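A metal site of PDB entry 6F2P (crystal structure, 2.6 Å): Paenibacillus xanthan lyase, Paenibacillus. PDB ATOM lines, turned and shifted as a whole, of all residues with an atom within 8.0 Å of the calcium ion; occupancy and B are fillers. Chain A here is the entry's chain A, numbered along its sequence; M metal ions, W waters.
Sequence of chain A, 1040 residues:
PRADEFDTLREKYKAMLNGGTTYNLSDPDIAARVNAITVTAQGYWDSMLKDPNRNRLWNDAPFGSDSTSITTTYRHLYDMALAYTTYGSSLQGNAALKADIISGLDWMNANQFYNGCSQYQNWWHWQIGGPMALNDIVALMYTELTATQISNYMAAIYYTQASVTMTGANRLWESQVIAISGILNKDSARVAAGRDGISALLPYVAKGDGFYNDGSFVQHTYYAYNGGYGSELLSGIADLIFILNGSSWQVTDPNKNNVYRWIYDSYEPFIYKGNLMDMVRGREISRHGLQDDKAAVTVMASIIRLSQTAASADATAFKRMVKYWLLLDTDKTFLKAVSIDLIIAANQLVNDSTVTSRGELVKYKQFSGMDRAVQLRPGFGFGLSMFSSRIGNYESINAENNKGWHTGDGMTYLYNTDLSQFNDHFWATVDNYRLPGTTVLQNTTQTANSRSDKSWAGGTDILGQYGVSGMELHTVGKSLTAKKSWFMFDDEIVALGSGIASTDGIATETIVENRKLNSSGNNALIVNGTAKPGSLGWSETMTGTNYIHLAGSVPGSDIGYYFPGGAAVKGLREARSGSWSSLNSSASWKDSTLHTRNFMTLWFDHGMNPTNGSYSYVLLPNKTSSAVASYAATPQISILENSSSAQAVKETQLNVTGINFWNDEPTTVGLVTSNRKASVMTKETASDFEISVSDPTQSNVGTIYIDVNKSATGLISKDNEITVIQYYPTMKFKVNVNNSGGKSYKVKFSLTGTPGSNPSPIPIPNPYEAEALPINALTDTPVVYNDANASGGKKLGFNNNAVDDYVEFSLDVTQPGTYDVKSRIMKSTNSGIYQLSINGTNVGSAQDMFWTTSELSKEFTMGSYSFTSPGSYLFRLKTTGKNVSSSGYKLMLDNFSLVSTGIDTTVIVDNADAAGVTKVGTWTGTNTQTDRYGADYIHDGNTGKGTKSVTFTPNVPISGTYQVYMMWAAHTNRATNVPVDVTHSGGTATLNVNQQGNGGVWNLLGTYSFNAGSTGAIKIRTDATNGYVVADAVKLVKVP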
ATOM      1  N   LYS A 273      21.193 -18.506 -10.759  1.00  0.00           N
ATOM      2  CA  LYS A 273      20.260 -19.022  -9.763  1.00  0.00           C
ATOM      3  C   LYS A 273      19.185 -18.008  -9.344  1.00  0.00           C
ATOM      4  O   LYS A 273      18.917 -17.824  -8.157  1.00  0.00           O
ATOM      5  CB  LYS A 273      21.033 -19.561  -8.565  1.00  0.00           C
ATOM      6  CG  LYS A 273      21.990 -20.674  -8.939  1.00  0.00           C
ATOM      7  CD  LYS A 273      22.743 -21.197  -7.726  1.00  0.00           C
ATOM      8  CE  LYS A 273      23.587 -22.403  -8.096  1.00  0.00           C
ATOM      9  NZ  LYS A 273      24.219 -23.010  -6.898  1.00  0.00           N
ATOM     10  N   GLY A 274      18.612 -17.332 -10.327  1.00  0.00           N
ATOM     11  CA  GLY A 274      17.506 -16.424 -10.082  1.00  0.00           C
ATOM     12  C   GLY A 274      17.920 -14.979  -9.939  1.00  0.00           C
ATOM     13  O   GLY A 274      17.072 -14.108  -9.717  1.00  0.00           O
ATOM     14  N   ASN A 275      19.216 -14.734 -10.059  1.00  0.00           N
ATOM     15  CA  ASN A 275      19.759 -13.387  -9.933  1.00  0.00           C
ATOM     16  C   ASN A 275      20.263 -12.864 -11.278  1.00  0.00           C
ATOM     17  O   ASN A 275      21.172 -13.435 -11.868  1.00  0.00           O
ATOM     18  CB  ASN A 275      20.911 -13.391  -8.932  1.00  0.00           C
ATOM     19  CG  ASN A 275      20.460 -13.759  -7.539  1.00  0.00           C
ATOM     20  OD1 ASN A 275      19.429 -13.273  -7.071  1.00  0.00           O
ATOM     21  ND2 ASN A 275      21.227 -14.604  -6.876  1.00  0.00           N
ATOM     22  N   ASP A 293      17.542 -10.219  -7.855  1.00  0.00           N
ATOM     23  CA  ASP A 293      16.571 -11.310  -7.862  1.00  0.00           C
ATOM     24  C   ASP A 293      15.200 -10.880  -8.389  1.00  0.00           C
ATOM     25  O   ASP A 293      14.533 -11.651  -9.080  1.00  0.00           O
ATOM     26  CB  ASP A 293      16.435 -11.968  -6.484  1.00  0.00           C
ATOM     27  CG  ASP A 293      15.898 -11.025  -5.429  1.00  0.00           C
ATOM     28  OD1 ASP A 293      16.014  -9.788  -5.581  1.00  0.00           O
ATOM     29  OD2 ASP A 293      15.368 -11.536  -4.421  1.00  0.00           O
ATOM     30  N   LYS A 294      14.803  -9.642  -8.099  1.00  0.00           N
ATOM     31  CA  LYS A 294      13.547  -9.130  -8.657  1.00  0.00           C
ATOM     32  C   LYS A 294      13.709  -8.807 -10.142  1.00  0.00           C
ATOM     33  O   LYS A 294      12.779  -8.997 -10.923  1.00  0.00           O
ATOM     34  CB  LYS A 294      13.036  -7.897  -7.885  1.00  0.00           C
ATOM     35  CG  LYS A 294      12.105  -8.211  -6.717  1.00  0.00           C
ATOM     36  CD  LYS A 294      10.642  -8.308  -7.162  1.00  0.00           C
ATOM     37  CE  LYS A 294       9.701  -8.426  -5.960  1.00  0.00           C
ATOM     38  NZ  LYS A 294       8.262  -8.134  -6.308  1.00  0.00           N
ATOM     39  N   VAL A 297      13.029 -11.569 -12.747  1.00  0.00           N
ATOM     40  CA  VAL A 297      11.669 -12.053 -12.927  1.00  0.00           C
ATOM     41  C   VAL A 297      11.089 -11.793 -14.324  1.00  0.00           C
ATOM     42  O   VAL A 297      10.513 -12.690 -14.932  1.00  0.00           O
ATOM     43  CB  VAL A 297      10.717 -11.528 -11.832  1.00  0.00           C
ATOM     44  CG1 VAL A 297       9.285 -11.812 -12.191  1.00  0.00           C
ATOM     45  CG2 VAL A 297      11.065 -12.169 -10.486  1.00  0.00           C
ATOM     46  N   TRP A 325      15.616 -22.648 -12.385  1.00  0.00           N
ATOM     47  CA  TRP A 325      15.566 -21.438 -11.592  1.00  0.00           C
ATOM     48  C   TRP A 325      14.364 -21.379 -10.646  1.00  0.00           C
ATOM     49  O   TRP A 325      14.455 -20.814  -9.557  1.00  0.00           O
ATOM     50  CB  TRP A 325      15.557 -20.202 -12.498  1.00  0.00           C
ATOM     51  CG  TRP A 325      16.813 -20.019 -13.284  1.00  0.00           C
ATOM     52  CD1 TRP A 325      18.099 -20.281 -12.878  1.00  0.00           C
ATOM     53  CD2 TRP A 325      16.918 -19.523 -14.631  1.00  0.00           C
ATOM     54  NE1 TRP A 325      18.986 -19.974 -13.894  1.00  0.00           N
ATOM     55  CE2 TRP A 325      18.290 -19.517 -14.976  1.00  0.00           C
ATOM     56  CE3 TRP A 325      15.984 -19.096 -15.584  1.00  0.00           C
ATOM     57  CZ2 TRP A 325      18.737 -19.082 -16.221  1.00  0.00           C
ATOM     58  CZ3 TRP A 325      16.433 -18.670 -16.818  1.00  0.00           C
ATOM     59  CH2 TRP A 325      17.793 -18.670 -17.131  1.00  0.00           C
ATOM     60  N   LEU A 326      13.236 -21.959 -11.050  1.00  0.00           N
ATOM     61  CA  LEU A 326      12.031 -21.897 -10.235  1.00  0.00           C
ATOM     62  C   LEU A 326      12.162 -22.824  -9.045  1.00  0.00           C
ATOM     63  O   LEU A 326      11.708 -22.501  -7.946  1.00  0.00           O
ATOM     64  CB  LEU A 326      10.798 -22.295 -11.050  1.00  0.00           C
ATOM     65  CG  LEU A 326      10.272 -21.250 -12.025  1.00  0.00           C
ATOM     66  CD1 LEU A 326       9.229 -21.882 -12.951  1.00  0.00           C
ATOM     67  CD2 LEU A 326       9.681 -20.096 -11.259  1.00  0.00           C
ATOM     68  N   LEU A 328      14.853 -23.440  -7.550  1.00  0.00           N
ATOM     69  CA  LEU A 328      15.795 -22.831  -6.639  1.00  0.00           C
ATOM     70  C   LEU A 328      15.120 -21.740  -5.840  1.00  0.00           C
ATOM     71  O   LEU A 328      15.564 -21.387  -4.756  1.00  0.00           O
ATOM     72  CB  LEU A 328      16.996 -22.264  -7.395  1.00  0.00           C
ATOM     73  CG  LEU A 328      17.911 -23.309  -8.007  1.00  0.00           C
ATOM     74  CD1 LEU A 328      18.937 -22.666  -8.908  1.00  0.00           C
ATOM     75  CD2 LEU A 328      18.589 -24.102  -6.929  1.00  0.00           C
ATOM     76  N   ASP A 329      14.026 -21.214  -6.389  1.00  0.00           N
ATOM     77  CA  ASP A 329      13.339 -20.057  -5.824  1.00  0.00           C
ATOM     78  C   ASP A 329      12.442 -20.432  -4.644  1.00  0.00           C
ATOM     79  O   ASP A 329      11.221 -20.279  -4.694  1.00  0.00           O
ATOM     80  CB  ASP A 329      12.543 -19.335  -6.907  1.00  0.00           C
ATOM     81  CG  ASP A 329      12.199 -17.904  -6.529  1.00  0.00           C
ATOM     82  OD1 ASP A 329      12.751 -17.421  -5.518  1.00  0.00           O
ATOM     83  OD2 ASP A 329      11.392 -17.261  -7.252  1.00  0.00           O
ATOM     84  N   THR A 330      13.076 -20.934  -3.580  1.00  0.00           N
ATOM     85  CA  THR A 330      12.387 -21.426  -2.388  1.00  0.00           C
ATOM     86  C   THR A 330      11.485 -20.393  -1.724  1.00  0.00           C
ATOM     87  O   THR A 330      10.493 -20.761  -1.099  1.00  0.00           O
ATOM     88  CB  THR A 330      13.410 -21.934  -1.363  1.00  0.00           C
ATOM     89  OG1 THR A 330      14.270 -20.858  -0.962  1.00  0.00           O
ATOM     90  CG2 THR A 330      14.267 -23.049  -1.960  1.00  0.00           C
ATOM     91  N   ASP A 331      11.816 -19.116  -1.842  1.00  0.00           N
ATOM     92  CA  ASP A 331      10.994 -18.067  -1.246  1.00  0.00           C
ATOM     93  C   ASP A 331      10.032 -17.434  -2.262  1.00  0.00           C
ATOM     94  O   ASP A 331       9.483 -16.360  -2.026  1.00  0.00           O
ATOM     95  CB  ASP A 331      11.865 -16.979  -0.596  1.00  0.00           C
ATOM     96  CG  ASP A 331      12.751 -16.261  -1.594  1.00  0.00           C
ATOM     97  OD1 ASP A 331      12.903 -16.769  -2.729  1.00  0.00           O
ATOM     98  OD2 ASP A 331      13.298 -15.204  -1.244  1.00  0.00           O
ATOM     99  N   LYS A 332       9.862 -18.115  -3.395  1.00  0.00           N
ATOM    100  CA  LYS A 332       8.867 -17.735  -4.404  1.00  0.00           C
ATOM    101  C   LYS A 332       8.934 -16.274  -4.896  1.00  0.00           C
ATOM    102  O   LYS A 332       7.906 -15.630  -5.112  1.00  0.00           O
ATOM    103  CB  LYS A 332       7.458 -18.081  -3.902  1.00  0.00           C
ATOM    104  CG  LYS A 332       7.277 -19.566  -3.648  1.00  0.00           C
ATOM    105  CD  LYS A 332       5.868 -19.905  -3.194  1.00  0.00           C
ATOM    106  CE  LYS A 332       5.682 -21.410  -3.132  1.00  0.00           C
ATOM    107  NZ  LYS A 332       4.317 -21.770  -2.673  1.00  0.00           N
ATOM    108  N   THR A 333      10.159 -15.779  -5.085  1.00  0.00           N
ATOM    109  CA  THR A 333      10.378 -14.477  -5.698  1.00  0.00           C
ATOM    110  C   THR A 333       9.545 -14.323  -6.968  1.00  0.00           C
ATOM    111  O   THR A 333       8.801 -13.363  -7.109  1.00  0.00           O
ATOM    112  CB  THR A 333      11.872 -14.261  -6.040  1.00  0.00           C
ATOM    113  OG1 THR A 333      12.663 -14.397  -4.849  1.00  0.00           O
ATOM    114  CG2 THR A 333      12.088 -12.877  -6.625  1.00  0.00           C
ATOM    115  N   PHE A 334       9.668 -15.294  -7.881  1.00  0.00           N
ATOM    116  CA  PHE A 334       8.909 -15.267  -9.131  1.00  0.00           C
ATOM    117  C   PHE A 334       7.393 -15.366  -8.930  1.00  0.00           C
ATOM    118  O   PHE A 334       6.650 -14.481  -9.378  1.00  0.00           O
ATOM    119  CB  PHE A 334       9.386 -16.380 -10.085  1.00  0.00           C
ATOM    120  CG  PHE A 334       8.651 -16.382 -11.413  1.00  0.00           C
ATOM    121  CD1 PHE A 334       9.091 -15.585 -12.453  1.00  0.00           C
ATOM    122  CD2 PHE A 334       7.538 -17.168 -11.610  1.00  0.00           C
ATOM    123  CE1 PHE A 334       8.423 -15.583 -13.670  1.00  0.00           C
ATOM    124  CE2 PHE A 334       6.869 -17.160 -12.814  1.00  0.00           C
ATOM    125  CZ  PHE A 334       7.305 -16.380 -13.839  1.00  0.00           C
ATOM    126  N   LEU A 419      22.338 -16.776  -2.301  1.00  0.00           N
ATOM    127  CA  LEU A 419      21.502 -16.160  -3.345  1.00  0.00           C
ATOM    128  C   LEU A 419      21.179 -14.701  -3.091  1.00  0.00           C
ATOM    129  O   LEU A 419      20.880 -13.954  -4.032  1.00  0.00           O
ATOM    130  CB  LEU A 419      20.202 -16.951  -3.533  1.00  0.00           C
ATOM    131  CG  LEU A 419      20.345 -18.447  -3.858  1.00  0.00           C
ATOM    132  CD1 LEU A 419      19.005 -19.024  -4.236  1.00  0.00           C
ATOM    133  CD2 LEU A 419      21.367 -18.668  -4.961  1.00  0.00           C
ATOM    134  N   SER A 420      21.237 -14.273  -1.835  1.00  0.00           N
ATOM    135  CA  SER A 420      20.775 -12.937  -1.498  1.00  0.00           C
ATOM    136  C   SER A 420      21.917 -11.926  -1.428  1.00  0.00           C
ATOM    137  O   SER A 420      21.689 -10.753  -1.134  1.00  0.00           O
ATOM    138  CB  SER A 420      20.011 -12.947  -0.163  1.00  0.00           C
ATOM    139  OG  SER A 420      20.920 -13.041   0.922  1.00  0.00           O
ATOM    140  N   ASN A 423      21.290  -8.782  -3.283  1.00  0.00           N
ATOM    141  CA  ASN A 423      20.001  -8.188  -2.927  1.00  0.00           C
ATOM    142  C   ASN A 423      19.918  -8.052  -1.406  1.00  0.00           C
ATOM    143  O   ASN A 423      20.949  -7.995  -0.746  1.00  0.00           O
ATOM    144  CB  ASN A 423      18.823  -8.958  -3.542  1.00  0.00           C
ATOM    145  CG  ASN A 423      18.941 -10.466  -3.374  1.00  0.00           C
ATOM    146  OD1 ASN A 423      18.513 -11.018  -2.363  1.00  0.00           O
ATOM    147  ND2 ASN A 423      19.529 -11.133  -4.375  1.00  0.00           N
HETATM  148 CA    CA M   1      14.334 -15.941  -4.373  1.00  0.00          CA
HETATM  149  O   HOH W   1      15.482 -18.051  -4.466  1.00  0.00           O
HETATM  150  O   HOH W   2      15.139 -15.525  -6.573  1.00  0.00           O
HETATM  151  O   HOH W   3      15.776 -14.091  -2.931  1.00  0.00           O
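The calcium ion is bound by the side-chain hydroxyl (OG1) of Thr 333, the side-chain carboxylate (OD1) of Asp 331, water W2, water W1, the side-chain carboxylate (OD1) of Asp 329 and water W3.
The side-chain carboxylate (OD2) of Asp 329 is in hydrogen-bond range of the backbone NH (N) of Phe 334, 2.7 Å away.
Water W3 lies within hydrogen-bond range of OD2 of Asp 293 and OD2 of Asp 331.
Three residues have an atom within 4 Å of the calcium ion: Asp 329, Asp 331 and Thr 333.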
